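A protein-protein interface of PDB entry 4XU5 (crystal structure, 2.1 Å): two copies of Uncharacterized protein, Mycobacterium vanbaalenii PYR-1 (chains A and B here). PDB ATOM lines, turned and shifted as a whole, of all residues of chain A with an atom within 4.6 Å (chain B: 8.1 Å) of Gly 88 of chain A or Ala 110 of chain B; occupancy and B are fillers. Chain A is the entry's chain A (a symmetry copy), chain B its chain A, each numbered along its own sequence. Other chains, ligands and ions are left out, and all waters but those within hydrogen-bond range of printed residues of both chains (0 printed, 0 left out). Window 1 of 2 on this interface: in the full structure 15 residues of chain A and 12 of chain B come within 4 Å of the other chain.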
ATOM      1  N   ALA A  84     -15.492  12.055   1.091  1.00  0.00           N
ATOM      2  CA  ALA A  84     -15.723  13.132   0.132  1.00  0.00           C
ATOM      3  C   ALA A  84     -17.211  13.482   0.094  1.00  0.00           C
ATOM      4  O   ALA A  84     -17.589  14.658   0.108  1.00  0.00           O
ATOM      5  CB  ALA A  84     -15.214  12.735  -1.260  1.00  0.00           C
ATOM      6  N   ALA A  85     -18.050  12.452   0.076  1.00  0.00           N
ATOM      7  CA  ALA A  85     -19.497  12.664   0.064  1.00  0.00           C
ATOM      8  C   ALA A  85     -19.969  13.429   1.303  1.00  0.00           C
ATOM      9  O   ALA A  85     -20.785  14.344   1.204  1.00  0.00           O
ATOM     10  CB  ALA A  85     -20.225  11.325  -0.036  1.00  0.00           C
ATOM     11  N   VAL A  86     -19.473  13.031   2.468  1.00  0.00           N
ATOM     12  CA  VAL A  86     -19.873  13.675   3.716  1.00  0.00           C
ATOM     13  C   VAL A  86     -19.371  15.121   3.784  1.00  0.00           C
ATOM     14  O   VAL A  86     -20.120  16.020   4.147  1.00  0.00           O
ATOM     15  CB  VAL A  86     -19.401  12.871   4.955  1.00  0.00           C
ATOM     16  CG1 VAL A  86     -19.487  13.734   6.233  1.00  0.00           C
ATOM     17  CG2 VAL A  86     -20.237  11.592   5.090  1.00  0.00           C
ATOM     18  N   VAL A  87     -18.115  15.334   3.412  1.00  0.00           N
ATOM     19  CA  VAL A  87     -17.548  16.691   3.376  1.00  0.00           C
ATOM     20  C   VAL A  87     -18.257  17.569   2.334  1.00  0.00           C
ATOM     21  O   VAL A  87     -18.627  18.713   2.619  1.00  0.00           O
ATOM     22  CB  VAL A  87     -16.024  16.664   3.093  1.00  0.00           C
ATOM     23  CG1 VAL A  87     -15.488  18.076   2.870  1.00  0.00           C
ATOM     24  CG2 VAL A  87     -15.278  15.994   4.256  1.00  0.00           C
ATOM     25  N   GLY A  88     -18.449  17.020   1.131  1.00  0.00           N
ATOM     26  CA  GLY A  88     -19.175  17.712   0.074  1.00  0.00           C
ATOM     27  C   GLY A  88     -20.562  18.137   0.531  1.00  0.00           C
ATOM     28  O   GLY A  88     -20.978  19.269   0.304  1.00  0.00           O
ATOM     29  N   THR A  89     -21.278  17.227   1.186  1.00  0.00           N
ATOM     30  CA  THR A  89     -22.618  17.540   1.671  1.00  0.00           C
ATOM     31  C   THR A  89     -22.558  18.619   2.768  1.00  0.00           C
ATOM     32  O   THR A  89     -23.346  19.563   2.774  1.00  0.00           O
ATOM     33  CB  THR A  89     -23.333  16.270   2.189  1.00  0.00           C
ATOM     34  OG1 THR A  89     -23.352  15.274   1.156  1.00  0.00           O
ATOM     35  CG2 THR A  89     -24.775  16.586   2.611  1.00  0.00           C
ATOM     36  N   TYR A  90     -21.602  18.470   3.681  1.00  0.00           N
ATOM     37  CA  TYR A  90     -21.389  19.417   4.780  1.00  0.00           C
ATOM     38  C   TYR A  90     -21.200  20.844   4.230  1.00  0.00           C
ATOM     39  O   TYR A  90     -21.928  21.769   4.610  1.00  0.00           O
ATOM     40  CB  TYR A  90     -20.150  18.969   5.570  1.00  0.00           C
ATOM     41  CG  TYR A  90     -19.947  19.548   6.961  1.00  0.00           C
ATOM     42  CD1 TYR A  90     -20.653  20.666   7.414  1.00  0.00           C
ATOM     43  CD2 TYR A  90     -19.037  18.956   7.827  1.00  0.00           C
ATOM     44  CE1 TYR A  90     -20.446  21.167   8.702  1.00  0.00           C
ATOM     45  CE2 TYR A  90     -18.831  19.443   9.104  1.00  0.00           C
ATOM     46  CZ  TYR A  90     -19.525  20.540   9.534  1.00  0.00           C
ATOM     47  OH  TYR A  90     -19.267  20.982  10.802  1.00  0.00           O
ATOM     48  N   VAL A  91     -20.248  21.021   3.317  1.00  0.00           N
ATOM     49  CA  VAL A  91     -19.985  22.363   2.798  1.00  0.00           C
ATOM     50  C   VAL A  91     -21.147  22.863   1.963  1.00  0.00           C
ATOM     51  O   VAL A  91     -21.375  24.060   1.884  1.00  0.00           O
ATOM     52  CB  VAL A  91     -18.634  22.500   2.022  1.00  0.00           C
ATOM     53  CG1 VAL A  91     -17.436  22.226   2.946  1.00  0.00           C
ATOM     54  CG2 VAL A  91     -18.591  21.591   0.797  1.00  0.00           C
ATOM     55  N   THR A  92     -21.894  21.947   1.351  1.00  0.00           N
ATOM     56  CA  THR A  92     -23.061  22.358   0.563  1.00  0.00           C
ATOM     57  C   THR A  92     -24.136  23.001   1.456  1.00  0.00           C
ATOM     58  O   THR A  92     -24.795  23.963   1.048  1.00  0.00           O
ATOM     59  CB  THR A  92     -23.650  21.173  -0.263  1.00  0.00           C
ATOM     60  OG1 THR A  92     -22.696  20.754  -1.262  1.00  0.00           O
ATOM     61  CG2 THR A  92     -24.962  21.582  -0.956  1.00  0.00           C
ATOM     62  N   THR B  89     -19.392  19.470 -12.643  1.00  0.00           N
ATOM     63  CA  THR B  89     -18.533  20.160 -11.687  1.00  0.00           C
ATOM     64  C   THR B  89     -18.107  21.534 -12.235  1.00  0.00           C
ATOM     65  O   THR B  89     -18.128  22.537 -11.524  1.00  0.00           O
ATOM     66  CB  THR B  89     -17.296  19.303 -11.332  1.00  0.00           C
ATOM     67  OG1 THR B  89     -17.720  18.021 -10.848  1.00  0.00           O
ATOM     68  CG2 THR B  89     -16.443  19.992 -10.256  1.00  0.00           C
ATOM     69  N   PRO B 103     -15.542  26.577   1.455  1.00  0.00           N
ATOM     70  CA  PRO B 103     -16.580  25.603   1.085  1.00  0.00           C
ATOM     71  C   PRO B 103     -16.616  25.355  -0.417  1.00  0.00           C
ATOM     72  O   PRO B 103     -16.888  24.234  -0.821  1.00  0.00           O
ATOM     73  CB  PRO B 103     -17.884  26.267   1.549  1.00  0.00           C
ATOM     74  CG  PRO B 103     -17.535  27.757   1.707  1.00  0.00           C
ATOM     75  CD  PRO B 103     -16.109  27.759   2.146  1.00  0.00           C
ATOM     76  N   VAL B 104     -16.340  26.380  -1.222  1.00  0.00           N
ATOM     77  CA  VAL B 104     -16.344  26.220  -2.672  1.00  0.00           C
ATOM     78  C   VAL B 104     -15.264  25.242  -3.134  1.00  0.00           C
ATOM     79  O   VAL B 104     -15.538  24.307  -3.887  1.00  0.00           O
ATOM     80  CB  VAL B 104     -16.159  27.576  -3.408  1.00  0.00           C
ATOM     81  CG1 VAL B 104     -15.904  27.346  -4.902  1.00  0.00           C
ATOM     82  CG2 VAL B 104     -17.370  28.463  -3.195  1.00  0.00           C
ATOM     83  N   THR B 105     -14.036  25.474  -2.691  1.00  0.00           N
ATOM     84  CA  THR B 105     -12.918  24.625  -3.087  1.00  0.00           C
ATOM     85  C   THR B 105     -13.086  23.190  -2.565  1.00  0.00           C
ATOM     86  O   THR B 105     -12.825  22.223  -3.286  1.00  0.00           O
ATOM     87  CB  THR B 105     -11.580  25.210  -2.611  1.00  0.00           C
ATOM     88  OG1 THR B 105     -11.467  26.570  -3.064  1.00  0.00           O
ATOM     89  CG2 THR B 105     -10.416  24.385  -3.156  1.00  0.00           C
ATOM     90  N   ALA B 106     -13.538  23.073  -1.318  1.00  0.00           N
ATOM     91  CA  ALA B 106     -13.828  21.775  -0.714  1.00  0.00           C
ATOM     92  C   ALA B 106     -14.908  21.028  -1.494  1.00  0.00           C
ATOM     93  O   ALA B 106     -14.832  19.802  -1.675  1.00  0.00           O
ATOM     94  CB  ALA B 106     -14.257  21.954   0.747  1.00  0.00           C
ATOM     95  N   LEU B 107     -15.922  21.757  -1.953  1.00  0.00           N
ATOM     96  CA  LEU B 107     -16.990  21.115  -2.717  1.00  0.00           C
ATOM     97  C   LEU B 107     -16.428  20.519  -4.005  1.00  0.00           C
ATOM     98  O   LEU B 107     -16.758  19.402  -4.390  1.00  0.00           O
ATOM     99  CB  LEU B 107     -18.112  22.105  -3.033  1.00  0.00           C
ATOM    100  CG  LEU B 107     -19.207  21.560  -3.961  1.00  0.00           C
ATOM    101  CD1 LEU B 107     -19.874  20.315  -3.374  1.00  0.00           C
ATOM    102  CD2 LEU B 107     -20.238  22.643  -4.249  1.00  0.00           C
ATOM    103  N   VAL B 108     -15.563  21.270  -4.669  1.00  0.00           N
ATOM    104  CA  VAL B 108     -15.020  20.805  -5.935  1.00  0.00           C
ATOM    105  C   VAL B 108     -14.027  19.651  -5.730  1.00  0.00           C
ATOM    106  O   VAL B 108     -13.970  18.724  -6.547  1.00  0.00           O
ATOM    107  CB  VAL B 108     -14.397  21.960  -6.746  1.00  0.00           C
ATOM    108  CG1 VAL B 108     -13.771  21.433  -8.047  1.00  0.00           C
ATOM    109  CG2 VAL B 108     -15.469  23.031  -7.041  1.00  0.00           C
ATOM    110  N   CYS B 109     -13.276  19.702  -4.631  1.00  0.00           N
ATOM    111  CA  CYS B 109     -12.374  18.606  -4.265  1.00  0.00           C
ATOM    112  C   CYS B 109     -13.153  17.314  -4.044  1.00  0.00           C
ATOM    113  O   CYS B 109     -12.704  16.225  -4.417  1.00  0.00           O
ATOM    114  CB  CYS B 109     -11.610  18.942  -2.984  1.00  0.00           C
ATOM    115  SG  CYS B 109     -10.278  20.096  -3.218  1.00  0.00           S
ATOM    116  N   ALA B 110     -14.314  17.455  -3.406  1.00  0.00           N
ATOM    117  CA  ALA B 110     -15.199  16.333  -3.139  1.00  0.00           C
ATOM    118  C   ALA B 110     -15.688  15.705  -4.442  1.00  0.00           C
ATOM    119  O   ALA B 110     -15.670  14.490  -4.591  1.00  0.00           O
ATOM    120  CB  ALA B 110     -16.378  16.782  -2.278  1.00  0.00           C
ATOM    121  N   ALA B 111     -16.118  16.540  -5.383  1.00  0.00           N
ATOM    122  CA  ALA B 111     -16.562  16.042  -6.678  1.00  0.00           C
ATOM    123  C   ALA B 111     -15.423  15.333  -7.432  1.00  0.00           C
ATOM    124  O   ALA B 111     -15.622  14.273  -8.023  1.00  0.00           O
ATOM    125  CB  ALA B 111     -17.150  17.170  -7.505  1.00  0.00           C
ATOM    126  N   ALA B 112     -14.236  15.929  -7.402  1.00  0.00           N
ATOM    127  CA  ALA B 112     -13.072  15.361  -8.064  1.00  0.00           C
ATOM    128  C   ALA B 112     -12.695  14.023  -7.445  1.00  0.00           C
ATOM    129  O   ALA B 112     -12.382  13.063  -8.159  1.00  0.00           O
ATOM    130  CB  ALA B 112     -11.891  16.325  -7.994  1.00  0.00           C
ATOM    131  N   ALA B 113     -12.734  13.956  -6.116  1.00  0.00           N
ATOM    132  CA  ALA B 113     -12.387  12.719  -5.408  1.00  0.00           C
ATOM    133  C   ALA B 113     -13.385  11.609  -5.732  1.00  0.00           C
ATOM    134  O   ALA B 113     -13.008  10.484  -6.060  1.00  0.00           O
ATOM    135  CB  ALA B 113     -12.323  12.956  -3.899  1.00  0.00           C
ATOM    136  N   ILE B 114     -14.671  11.931  -5.645  1.00  0.00           N
ATOM    137  CA  ILE B 114     -15.692  10.937  -5.936  1.00  0.00           C
ATOM    138  C   ILE B 114     -15.557  10.449  -7.385  1.00  0.00           C
ATOM    139  O   ILE B 114     -15.666   9.258  -7.650  1.00  0.00           O
ATOM    140  CB  ILE B 114     -17.112  11.479  -5.657  1.00  0.00           C
ATOM    141  CG1 ILE B 114     -17.337  11.617  -4.151  1.00  0.00           C
ATOM    142  CG2 ILE B 114     -18.173  10.571  -6.244  1.00  0.00           C
ATOM    143  CD1 ILE B 114     -18.575  12.428  -3.801  1.00  0.00           C
ATOM    144  N   THR B 115     -15.306  11.373  -8.312  1.00  0.00           N
ATOM    145  CA  THR B 115     -15.104  11.015  -9.715  1.00  0.00           C
ATOM    146  C   THR B 115     -13.968   9.987  -9.860  1.00  0.00           C
ATOM    147  O   THR B 115     -14.124   8.961 -10.536  1.00  0.00           O
ATOM    148  CB  THR B 115     -14.843  12.281 -10.591  1.00  0.00           C
ATOM    149  OG1 THR B 115     -15.936  13.197 -10.442  1.00  0.00           O
ATOM    150  CG2 THR B 115     -14.691  11.921 -12.064  1.00  0.00           C
ATOM    151  N   TRP B 116     -12.844  10.242  -9.194  1.00  0.00           N
ATOM    152  CA  TRP B 116     -11.741   9.287  -9.216  1.00  0.00           C
ATOM    153  C   TRP B 116     -12.128   7.946  -8.571  1.00  0.00           C
ATOM    154  O   TRP B 116     -11.783   6.875  -9.081  1.00  0.00           O
ATOM    155  CB  TRP B 116     -10.483   9.838  -8.526  1.00  0.00           C
ATOM    156  CG  TRP B 116      -9.393   8.822  -8.614  1.00  0.00           C
ATOM    157  CD1 TRP B 116      -8.473   8.696  -9.610  1.00  0.00           C
ATOM    158  CD2 TRP B 116      -9.152   7.738  -7.705  1.00  0.00           C
ATOM    159  NE1 TRP B 116      -7.662   7.616  -9.373  1.00  0.00           N
ATOM    160  CE2 TRP B 116      -8.058   7.006  -8.211  1.00  0.00           C
ATOM    161  CE3 TRP B 116      -9.756   7.317  -6.514  1.00  0.00           C
ATOM    162  CZ2 TRP B 116      -7.549   5.867  -7.566  1.00  0.00           C
ATOM    163  CZ3 TRP B 116      -9.244   6.181  -5.865  1.00  0.00           C
ATOM    164  CH2 TRP B 116      -8.148   5.479  -6.395  1.00  0.00           C
ATOM    165  N   CYS B 117     -12.824   8.018  -7.437  1.00  0.00           N
ATOM    166  CA  CYS B 117     -13.244   6.818  -6.720  1.00  0.00           C
ATOM    167  C   CYS B 117     -14.088   5.914  -7.605  1.00  0.00           C
ATOM    168  O   CYS B 117     -13.928   4.691  -7.588  1.00  0.00           O
ATOM    169  CB  CYS B 117     -13.995   7.176  -5.425  1.00  0.00           C
ATOM    170  SG  CYS B 117     -12.898   7.793  -4.131  1.00  0.00           S
ATOM    171  N   PRO B 166      -8.673  21.014  -8.265  1.00  0.00           N
ATOM    172  CA  PRO B 166      -9.441  19.762  -8.329  1.00  0.00           C
ATOM    173  C   PRO B 166     -10.249  19.625  -9.636  1.00  0.00           C
ATOM    174  O   PRO B 166     -10.450  18.503 -10.106  1.00  0.00           O
ATOM    175  CB  PRO B 166     -10.361  19.839  -7.096  1.00  0.00           C
ATOM    176  CG  PRO B 166     -10.482  21.342  -6.810  1.00  0.00           C
ATOM    177  CD  PRO B 166      -9.145  21.912  -7.185  1.00  0.00           C
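The side-chain sulfur of Cys 117 of chain B is in hydrogen-bond range of the backbone carbonyl oxygen of Ala 113 of chain B, at 3.3 Å.
The side-chain hydroxyl of Thr 92 of chain A lies within hydrogen-bond range of the backbone carbonyl oxygen of Gly 88 of chain A, at 2.8 Å.
The side-chain hydroxyl (OG1) of Thr 89 of chain A is in hydrogen-bond range of the backbone carbonyl oxygen (O) of Ala 85 of chain A (2.7 Å).
Among the printed residues, merely in contact across the chains: Ala 84 of chain A with Ala 110 of chain B (3.4 Å), Ala 84 of chain A with Ala 113 of chain B (3.9 Å), Ala 84 of chain A with Ile 114 of chain B (3.8 Å), Ala 85 of chain A with Ile 114 of chain B (3.9 Å), Gly 88 of chain A with Leu 107 of chain B (3.98 Å), Gly 88 of chain A with Ala 110 of chain B (3.8 Å), Val 91 of chain A with Pro 103 of chain B (3.5 Å), Val 91 of chain A with Ala 106 of chain B (3.9 Å), Val 91 of chain A with Leu 107 of chain B (3.8 Å) and Thr 92 of chain A with Leu 107 of chain B (3.6 Å).
Of the printed residues of chain B, Ala 84 of chain A touches Ala 110, Ala 113 and Ile 114.
Val 86 of chain A touches none of the printed residues of chain B.
Printed residues of chain B within 4 Å of Val 91 of chain A: Pro 103 (3.5 Å), Ala 106 (3.9 Å) and Leu 107 (3.8 Å).
Thr 89 of chain B touches none of the printed residues of chain A.
Of the printed residues of chain A, Ala 106 of chain B touches Val 91.
Ala 110 of chain B touches just these residues of chain A: Ala 84 and Gly 88.
Of the printed residues of chain A, Ala 113 of chain B touches Ala 84.
The nearest printed residue of chain B that does not touch Gly 88 of chain A is Ala 106 of chain B (5.1 Å).
The nearest printed residue of chain A that does not touch Ile 114 of chain B is Val 86 of chain A (6.4 Å).
Of the 9 printed residues of chain A, 5 touch a printed residue of chain B.
Hydrophobic or aromatic side chains of chain A within 4 Å of the printed part of chain B: Ala 84 and Val 91.
Along chain A the printed residues that touch a printed residue of chain B span positions 84 to 92.
Of the 17 printed residues of chain B, 6 touch a printed residue of chain A.
Among the printed residues, 10 pairs touch across the chains.
Among the printed residues, no Asp or Glu carboxylate lies within 4 Å of a Lys or Arg side-chain nitrogen of the other chain.
1 position is printed for both chains.
Of the 10 pairs that touch across the chains among the printed residues, none has its exchanged pair printed and touching as well.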
